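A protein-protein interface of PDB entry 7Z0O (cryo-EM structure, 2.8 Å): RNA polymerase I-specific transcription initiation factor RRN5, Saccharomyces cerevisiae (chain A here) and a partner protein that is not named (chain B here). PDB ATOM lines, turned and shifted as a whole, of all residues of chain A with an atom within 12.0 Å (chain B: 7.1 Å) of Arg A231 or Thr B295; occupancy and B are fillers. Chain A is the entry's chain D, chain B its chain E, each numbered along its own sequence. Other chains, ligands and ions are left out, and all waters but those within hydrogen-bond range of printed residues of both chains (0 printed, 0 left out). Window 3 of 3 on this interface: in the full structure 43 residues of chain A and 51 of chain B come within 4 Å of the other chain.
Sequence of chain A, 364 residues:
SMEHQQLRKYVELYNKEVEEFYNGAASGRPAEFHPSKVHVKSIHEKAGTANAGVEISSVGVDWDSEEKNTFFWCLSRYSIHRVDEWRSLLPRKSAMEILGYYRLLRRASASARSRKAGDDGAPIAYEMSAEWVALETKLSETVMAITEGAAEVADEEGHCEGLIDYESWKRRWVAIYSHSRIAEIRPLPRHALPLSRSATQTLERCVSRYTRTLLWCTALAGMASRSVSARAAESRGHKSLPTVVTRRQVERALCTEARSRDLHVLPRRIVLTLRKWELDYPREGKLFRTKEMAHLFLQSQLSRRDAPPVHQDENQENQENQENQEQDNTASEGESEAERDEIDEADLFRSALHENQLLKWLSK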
ATOM      1  N   SER A 227     -32.730   8.690   0.886  1.00  0.00           N
ATOM      2  CA  SER A 227     -32.132   8.775   2.209  1.00  0.00           C
ATOM      3  C   SER A 227     -30.941   9.721   2.156  1.00  0.00           C
ATOM      4  O   SER A 227     -30.492  10.132   1.084  1.00  0.00           O
ATOM      5  CB  SER A 227     -31.695   7.396   2.718  1.00  0.00           C
ATOM      6  OG  SER A 227     -32.792   6.505   2.782  1.00  0.00           O
ATOM      7  N   VAL A 228     -30.431  10.069   3.332  1.00  0.00           N
ATOM      8  CA  VAL A 228     -29.283  10.958   3.465  1.00  0.00           C
ATOM      9  C   VAL A 228     -28.077  10.120   3.863  1.00  0.00           C
ATOM     10  O   VAL A 228     -28.133   9.366   4.841  1.00  0.00           O
ATOM     11  CB  VAL A 228     -29.543  12.070   4.493  1.00  0.00           C
ATOM     12  CG1 VAL A 228     -28.304  12.925   4.668  1.00  0.00           C
ATOM     13  CG2 VAL A 228     -30.721  12.921   4.063  1.00  0.00           C
ATOM     14  N   SER A 229     -26.994  10.253   3.104  1.00  0.00           N
ATOM     15  CA  SER A 229     -25.764   9.515   3.378  1.00  0.00           C
ATOM     16  C   SER A 229     -25.100  10.120   4.608  1.00  0.00           C
ATOM     17  O   SER A 229     -24.373  11.110   4.515  1.00  0.00           O
ATOM     18  CB  SER A 229     -24.840   9.560   2.168  1.00  0.00           C
ATOM     19  OG  SER A 229     -23.657   8.817   2.402  1.00  0.00           O
ATOM     20  N   ALA A 230     -25.358   9.524   5.773  1.00  0.00           N
ATOM     21  CA  ALA A 230     -24.828  10.068   7.019  1.00  0.00           C
ATOM     22  C   ALA A 230     -23.309   9.961   7.070  1.00  0.00           C
ATOM     23  O   ALA A 230     -22.618  10.938   7.378  1.00  0.00           O
ATOM     24  CB  ALA A 230     -25.457   9.349   8.212  1.00  0.00           C
ATOM     25  N   ARG A 231     -22.773   8.785   6.766  1.00  0.00           N
ATOM     26  CA  ARG A 231     -21.333   8.543   6.855  1.00  0.00           C
ATOM     27  C   ARG A 231     -20.667   8.779   5.501  1.00  0.00           C
ATOM     28  O   ARG A 231     -20.014   7.906   4.929  1.00  0.00           O
ATOM     29  CB  ARG A 231     -21.068   7.131   7.372  1.00  0.00           C
ATOM     30  CG  ARG A 231     -21.190   6.987   8.885  1.00  0.00           C
ATOM     31  CD  ARG A 231     -22.644   6.863   9.318  1.00  0.00           C
ATOM     32  NE  ARG A 231     -22.795   6.856  10.769  1.00  0.00           N
ATOM     33  CZ  ARG A 231     -22.981   5.765  11.497  1.00  0.00           C
ATOM     34  NH1 ARG A 231     -23.036   4.565  10.945  1.00  0.00           N
ATOM     35  NH2 ARG A 231     -23.118   5.880  12.815  1.00  0.00           N
ATOM     36  N   ALA A 232     -20.845   9.992   4.991  1.00  0.00           N
ATOM     37  CA  ALA A 232     -20.276  10.374   3.704  1.00  0.00           C
ATOM     38  C   ALA A 232     -18.770  10.579   3.816  1.00  0.00           C
ATOM     39  O   ALA A 232     -18.250  10.850   4.897  1.00  0.00           O
ATOM     40  CB  ALA A 232     -20.945  11.634   3.180  1.00  0.00           C
ATOM     41  N   SER A 240     -25.884  14.239  -3.030  1.00  0.00           N
ATOM     42  CA  SER A 240     -26.937  13.417  -3.610  1.00  0.00           C
ATOM     43  C   SER A 240     -27.631  12.583  -2.541  1.00  0.00           C
ATOM     44  O   SER A 240     -27.048  12.278  -1.503  1.00  0.00           O
ATOM     45  CB  SER A 240     -26.369  12.506  -4.697  1.00  0.00           C
ATOM     46  OG  SER A 240     -25.713  11.387  -4.129  1.00  0.00           O
ATOM     47  N   LEU A 241     -28.881  12.211  -2.804  1.00  0.00           N
ATOM     48  CA  LEU A 241     -29.666  11.415  -1.869  1.00  0.00           C
ATOM     49  C   LEU A 241     -29.875  10.022  -2.438  1.00  0.00           C
ATOM     50  O   LEU A 241     -30.687   9.853  -3.362  1.00  0.00           O
ATOM     51  CB  LEU A 241     -31.012  12.086  -1.591  1.00  0.00           C
ATOM     52  CG  LEU A 241     -30.950  13.537  -1.115  1.00  0.00           C
ATOM     53  CD1 LEU A 241     -32.343  14.064  -0.848  1.00  0.00           C
ATOM     54  CD2 LEU A 241     -30.084  13.656   0.123  1.00  0.00           C
ATOM     55  N   PRO A 242     -29.187   9.005  -1.934  1.00  0.00           N
ATOM     56  CA  PRO A 242     -29.323   7.659  -2.493  1.00  0.00           C
ATOM     57  C   PRO A 242     -30.623   6.995  -2.057  1.00  0.00           C
ATOM     58  O   PRO A 242     -31.354   7.485  -1.198  1.00  0.00           O
ATOM     59  CB  PRO A 242     -28.113   6.922  -1.919  1.00  0.00           C
ATOM     60  CG  PRO A 242     -27.849   7.611  -0.633  1.00  0.00           C
ATOM     61  CD  PRO A 242     -28.181   9.057  -0.860  1.00  0.00           C
ATOM     62  N   VAL A 244     -31.989   3.418  -0.470  1.00  0.00           N
ATOM     63  CA  VAL A 244     -31.467   2.338   0.355  1.00  0.00           C
ATOM     64  C   VAL A 244     -32.548   1.285   0.527  1.00  0.00           C
ATOM     65  O   VAL A 244     -33.679   1.605   0.906  1.00  0.00           O
ATOM     66  CB  VAL A 244     -30.985   2.854   1.723  1.00  0.00           C
ATOM     67  CG1 VAL A 244     -30.343   1.731   2.513  1.00  0.00           C
ATOM     68  CG2 VAL A 244     -30.010   4.000   1.536  1.00  0.00           C
ATOM     69  N   GLU B 290     -23.755  18.091  12.846  1.00  0.00           N
ATOM     70  CA  GLU B 290     -23.606  17.460  14.153  1.00  0.00           C
ATOM     71  C   GLU B 290     -24.537  16.265  14.292  1.00  0.00           C
ATOM     72  O   GLU B 290     -24.158  15.238  14.868  1.00  0.00           O
ATOM     73  CB  GLU B 290     -23.872  18.477  15.262  1.00  0.00           C
ATOM     74  CG  GLU B 290     -22.871  19.622  15.319  1.00  0.00           C
ATOM     75  CD  GLU B 290     -23.273  20.800  14.450  1.00  0.00           C
ATOM     76  OE1 GLU B 290     -24.155  20.631  13.582  1.00  0.00           O
ATOM     77  OE2 GLU B 290     -22.710  21.898  14.637  1.00  0.00           O
ATOM     78  N   LEU B 291     -25.763  16.383  13.779  1.00  0.00           N
ATOM     79  CA  LEU B 291     -26.712  15.279  13.866  1.00  0.00           C
ATOM     80  C   LEU B 291     -26.233  14.071  13.071  1.00  0.00           C
ATOM     81  O   LEU B 291     -26.336  12.931  13.539  1.00  0.00           O
ATOM     82  CB  LEU B 291     -28.086  15.732  13.375  1.00  0.00           C
ATOM     83  CG  LEU B 291     -29.166  14.656  13.281  1.00  0.00           C
ATOM     84  CD1 LEU B 291     -29.340  13.979  14.624  1.00  0.00           C
ATOM     85  CD2 LEU B 291     -30.476  15.255  12.811  1.00  0.00           C
ATOM     86  N   LEU B 292     -25.705  14.302  11.869  1.00  0.00           N
ATOM     87  CA  LEU B 292     -25.279  13.195  11.019  1.00  0.00           C
ATOM     88  C   LEU B 292     -24.084  12.460  11.615  1.00  0.00           C
ATOM     89  O   LEU B 292     -23.981  11.234  11.494  1.00  0.00           O
ATOM     90  CB  LEU B 292     -24.948  13.706   9.619  1.00  0.00           C
ATOM     91  CG  LEU B 292     -26.137  14.039   8.717  1.00  0.00           C
ATOM     92  CD1 LEU B 292     -25.676  14.227   7.284  1.00  0.00           C
ATOM     93  CD2 LEU B 292     -27.194  12.955   8.802  1.00  0.00           C
ATOM     94  N   SER B 293     -23.166  13.192  12.249  1.00  0.00           N
ATOM     95  CA  SER B 293     -21.969  12.561  12.797  1.00  0.00           C
ATOM     96  C   SER B 293     -22.304  11.616  13.944  1.00  0.00           C
ATOM     97  O   SER B 293     -21.707  10.541  14.063  1.00  0.00           O
ATOM     98  CB  SER B 293     -20.979  13.630  13.256  1.00  0.00           C
ATOM     99  OG  SER B 293     -20.363  14.259  12.146  1.00  0.00           O
ATOM    100  N   LYS B 294     -23.253  11.995  14.794  1.00  0.00           N
ATOM    101  CA  LYS B 294     -23.560  11.238  16.000  1.00  0.00           C
ATOM    102  C   LYS B 294     -24.632  10.177  15.795  1.00  0.00           C
ATOM    103  O   LYS B 294     -24.926   9.431  16.733  1.00  0.00           O
ATOM    104  CB  LYS B 294     -23.994  12.191  17.117  1.00  0.00           C
ATOM    105  CG  LYS B 294     -22.883  13.091  17.626  1.00  0.00           C
ATOM    106  CD  LYS B 294     -23.335  13.894  18.833  1.00  0.00           C
ATOM    107  CE  LYS B 294     -24.324  14.976  18.430  1.00  0.00           C
ATOM    108  NZ  LYS B 294     -24.585  15.931  19.540  1.00  0.00           N
ATOM    109  N   THR B 295     -25.220  10.084  14.606  1.00  0.00           N
ATOM    110  CA  THR B 295     -26.282   9.117  14.389  1.00  0.00           C
ATOM    111  C   THR B 295     -25.724   7.697  14.358  1.00  0.00           C
ATOM    112  O   THR B 295     -24.543   7.465  14.082  1.00  0.00           O
ATOM    113  CB  THR B 295     -27.035   9.417  13.092  1.00  0.00           C
ATOM    114  OG1 THR B 295     -28.284   8.717  13.094  1.00  0.00           O
ATOM    115  CG2 THR B 295     -26.225   8.981  11.885  1.00  0.00           C
ATOM    116  N   ARG B 296     -26.595   6.735  14.661  1.00  0.00           N
ATOM    117  CA  ARG B 296     -26.214   5.328  14.683  1.00  0.00           C
ATOM    118  C   ARG B 296     -26.397   4.666  13.322  1.00  0.00           C
ATOM    119  O   ARG B 296     -25.510   3.947  12.855  1.00  0.00           O
ATOM    120  CB  ARG B 296     -27.026   4.582  15.744  1.00  0.00           C
ATOM    121  CG  ARG B 296     -26.765   5.046  17.167  1.00  0.00           C
ATOM    122  CD  ARG B 296     -28.026   4.969  18.011  1.00  0.00           C
ATOM    123  NE  ARG B 296     -28.426   3.594  18.283  1.00  0.00           N
ATOM    124  CZ  ARG B 296     -29.612   3.245  18.763  1.00  0.00           C
ATOM    125  NH1 ARG B 296     -30.544   4.146  19.026  1.00  0.00           N
ATOM    126  NH2 ARG B 296     -29.870   1.959  18.981  1.00  0.00           N
ATOM    127  N   GLU B 297     -27.538   4.898  12.680  1.00  0.00           N
ATOM    128  CA  GLU B 297     -27.819   4.272  11.398  1.00  0.00           C
ATOM    129  C   GLU B 297     -26.932   4.853  10.303  1.00  0.00           C
ATOM    130  O   GLU B 297     -26.580   6.034  10.316  1.00  0.00           O
ATOM    131  CB  GLU B 297     -29.291   4.451  11.032  1.00  0.00           C
ATOM    132  CG  GLU B 297     -30.227   3.509  11.773  1.00  0.00           C
ATOM    133  CD  GLU B 297     -30.600   2.292  10.952  1.00  0.00           C
ATOM    134  OE1 GLU B 297     -31.754   2.222  10.482  1.00  0.00           O
ATOM    135  OE2 GLU B 297     -29.739   1.403  10.778  1.00  0.00           O
ATOM    136  N   ASP B 298     -26.566   3.997   9.347  1.00  0.00           N
ATOM    137  CA  ASP B 298     -25.722   4.434   8.240  1.00  0.00           C
ATOM    138  C   ASP B 298     -26.458   5.409   7.330  1.00  0.00           C
ATOM    139  O   ASP B 298     -25.861   6.365   6.823  1.00  0.00           O
ATOM    140  CB  ASP B 298     -25.231   3.224   7.449  1.00  0.00           C
ATOM    141  CG  ASP B 298     -23.930   3.494   6.722  1.00  0.00           C
ATOM    142  OD1 ASP B 298     -23.489   4.663   6.703  1.00  0.00           O
ATOM    143  OD2 ASP B 298     -23.347   2.538   6.170  1.00  0.00           O
ATOM    144  N   PHE B 299     -27.747   5.178   7.100  1.00  0.00           N
ATOM    145  CA  PHE B 299     -28.562   6.042   6.260  1.00  0.00           C
ATOM    146  C   PHE B 299     -29.804   6.464   7.027  1.00  0.00           C
ATOM    147  O   PHE B 299     -30.394   5.664   7.760  1.00  0.00           O
ATOM    148  CB  PHE B 299     -28.969   5.342   4.961  1.00  0.00           C
ATOM    149  CG  PHE B 299     -27.816   5.033   4.054  1.00  0.00           C
ATOM    150  CD1 PHE B 299     -27.347   5.980   3.163  1.00  0.00           C
ATOM    151  CD2 PHE B 299     -27.204   3.793   4.088  1.00  0.00           C
ATOM    152  CE1 PHE B 299     -26.289   5.697   2.327  1.00  0.00           C
ATOM    153  CE2 PHE B 299     -26.146   3.506   3.255  1.00  0.00           C
ATOM    154  CZ  PHE B 299     -25.688   4.459   2.373  1.00  0.00           C
ATOM    155  N   ILE B 300     -30.194   7.719   6.858  1.00  0.00           N
ATOM    156  CA  ILE B 300     -31.374   8.285   7.502  1.00  0.00           C
ATOM    157  C   ILE B 300     -32.392   8.606   6.414  1.00  0.00           C
ATOM    158  O   ILE B 300     -32.068   9.341   5.473  1.00  0.00           O
ATOM    159  CB  ILE B 300     -31.030   9.539   8.320  1.00  0.00           C
ATOM    160  CG1 ILE B 300     -30.064   9.189   9.450  1.00  0.00           C
ATOM    161  CG2 ILE B 300     -32.292  10.167   8.881  1.00  0.00           C
ATOM    162  CD1 ILE B 300     -29.689  10.369  10.315  1.00  0.00           C
ATOM    163  N   ARG B 310     -34.851  18.722  15.720  1.00  0.00           N
ATOM    164  CA  ARG B 310     -33.479  19.130  15.984  1.00  0.00           C
ATOM    165  C   ARG B 310     -32.852  19.877  14.816  1.00  0.00           C
ATOM    166  O   ARG B 310     -31.714  20.341  14.936  1.00  0.00           O
ATOM    167  CB  ARG B 310     -32.623  17.908  16.327  1.00  0.00           C
ATOM    168  CG  ARG B 310     -32.979  17.255  17.648  1.00  0.00           C
ATOM    169  CD  ARG B 310     -32.269  15.925  17.808  1.00  0.00           C
ATOM    170  NE  ARG B 310     -32.760  14.936  16.858  1.00  0.00           N
ATOM    171  CZ  ARG B 310     -32.228  13.735  16.688  1.00  0.00           C
ATOM    172  NH1 ARG B 310     -31.185  13.334  17.395  1.00  0.00           N
ATOM    173  NH2 ARG B 310     -32.755  12.914  15.784  1.00  0.00           N
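The backbone carbonyl oxygen (O) of Thr B295 is in hydrogen-bond range of the guanidinium group (NH2) of Arg A231, 2.5 Å away.
The backbone carbonyl oxygen (O) of Ile B300 is in hydrogen-bond range of the backbone NH (N) of Val A228, at 2.8 Å.
NH2 of Arg A231 lies within hydrogen-bond range of O of Arg B296 (3.1 Å).
N of Ala A230 lies close to O of Asp B298, 3.4 Å away.
The backbone carbonyl oxygen (O) of Pro A242 sits at hydrogen-bond distance from the backbone NH (N) of Ser A227, 2.8 Å away.
Among the printed residues, pairs that only touch across the chains: Ser A227 with Ile B300, Val A244 with Phe B299, Arg A231 with Asp B298, Val A228 with Phe B299, Ala A230 with Thr B295, Arg A231 with Glu B297, Pro A242 with Phe B299, Ser A229 with Phe B299 and Val A228 with Leu B292.
Arg A231 touches just these residues of chain B: Thr B295, Arg B296, Glu B297 and Asp B298.
Of chain A, only Ala A230 (3.8 Å) and Arg A231 (2.5 Å) come within 4 Å of Thr B295.
No residue of chain A comes within 4 Å of Leu B291.
Of chain A, only Val A228 comes within 4 Å of Leu B292.
No residue of chain A comes within 4 Å of Ser B293.
No residue of chain A comes within 4 Å of Lys B294.
Asp B298 touches just these residues of chain A: Ala A230 (3.3 Å) and Arg A231 (3.5 Å).
Of the printed residues of chain A, Ile B300 touches Ser A227 (3.3 Å) and Val A228 (2.8 Å).
Of the printed residues of chain A, Arg B296 touches Arg A231 (3.1 Å).
The nearest residue of chain A that does not touch Thr B295 is Val A228 (7.3 Å).
The nearest printed residue of chain B that does not touch Ala A230 is Leu B292 (4.05 Å).
Of the 12 printed residues of chain B, 7 touch a printed residue of chain A.
Printed residues of chain B that touch a printed residue of chain A: Leu B292, Thr B295, Arg B296, Glu B297, Asp B298, Phe B299 and Ile B300.
Of the 10 printed residues of chain A, 7 touch a printed residue of chain B.
Hydrophobic or aromatic side chains of chain A within 4 Å of the printed part of chain B: Val A228, Ala A230, Pro A242 and Val A244.
Among the printed residues, 13 pairs touch across the chains.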
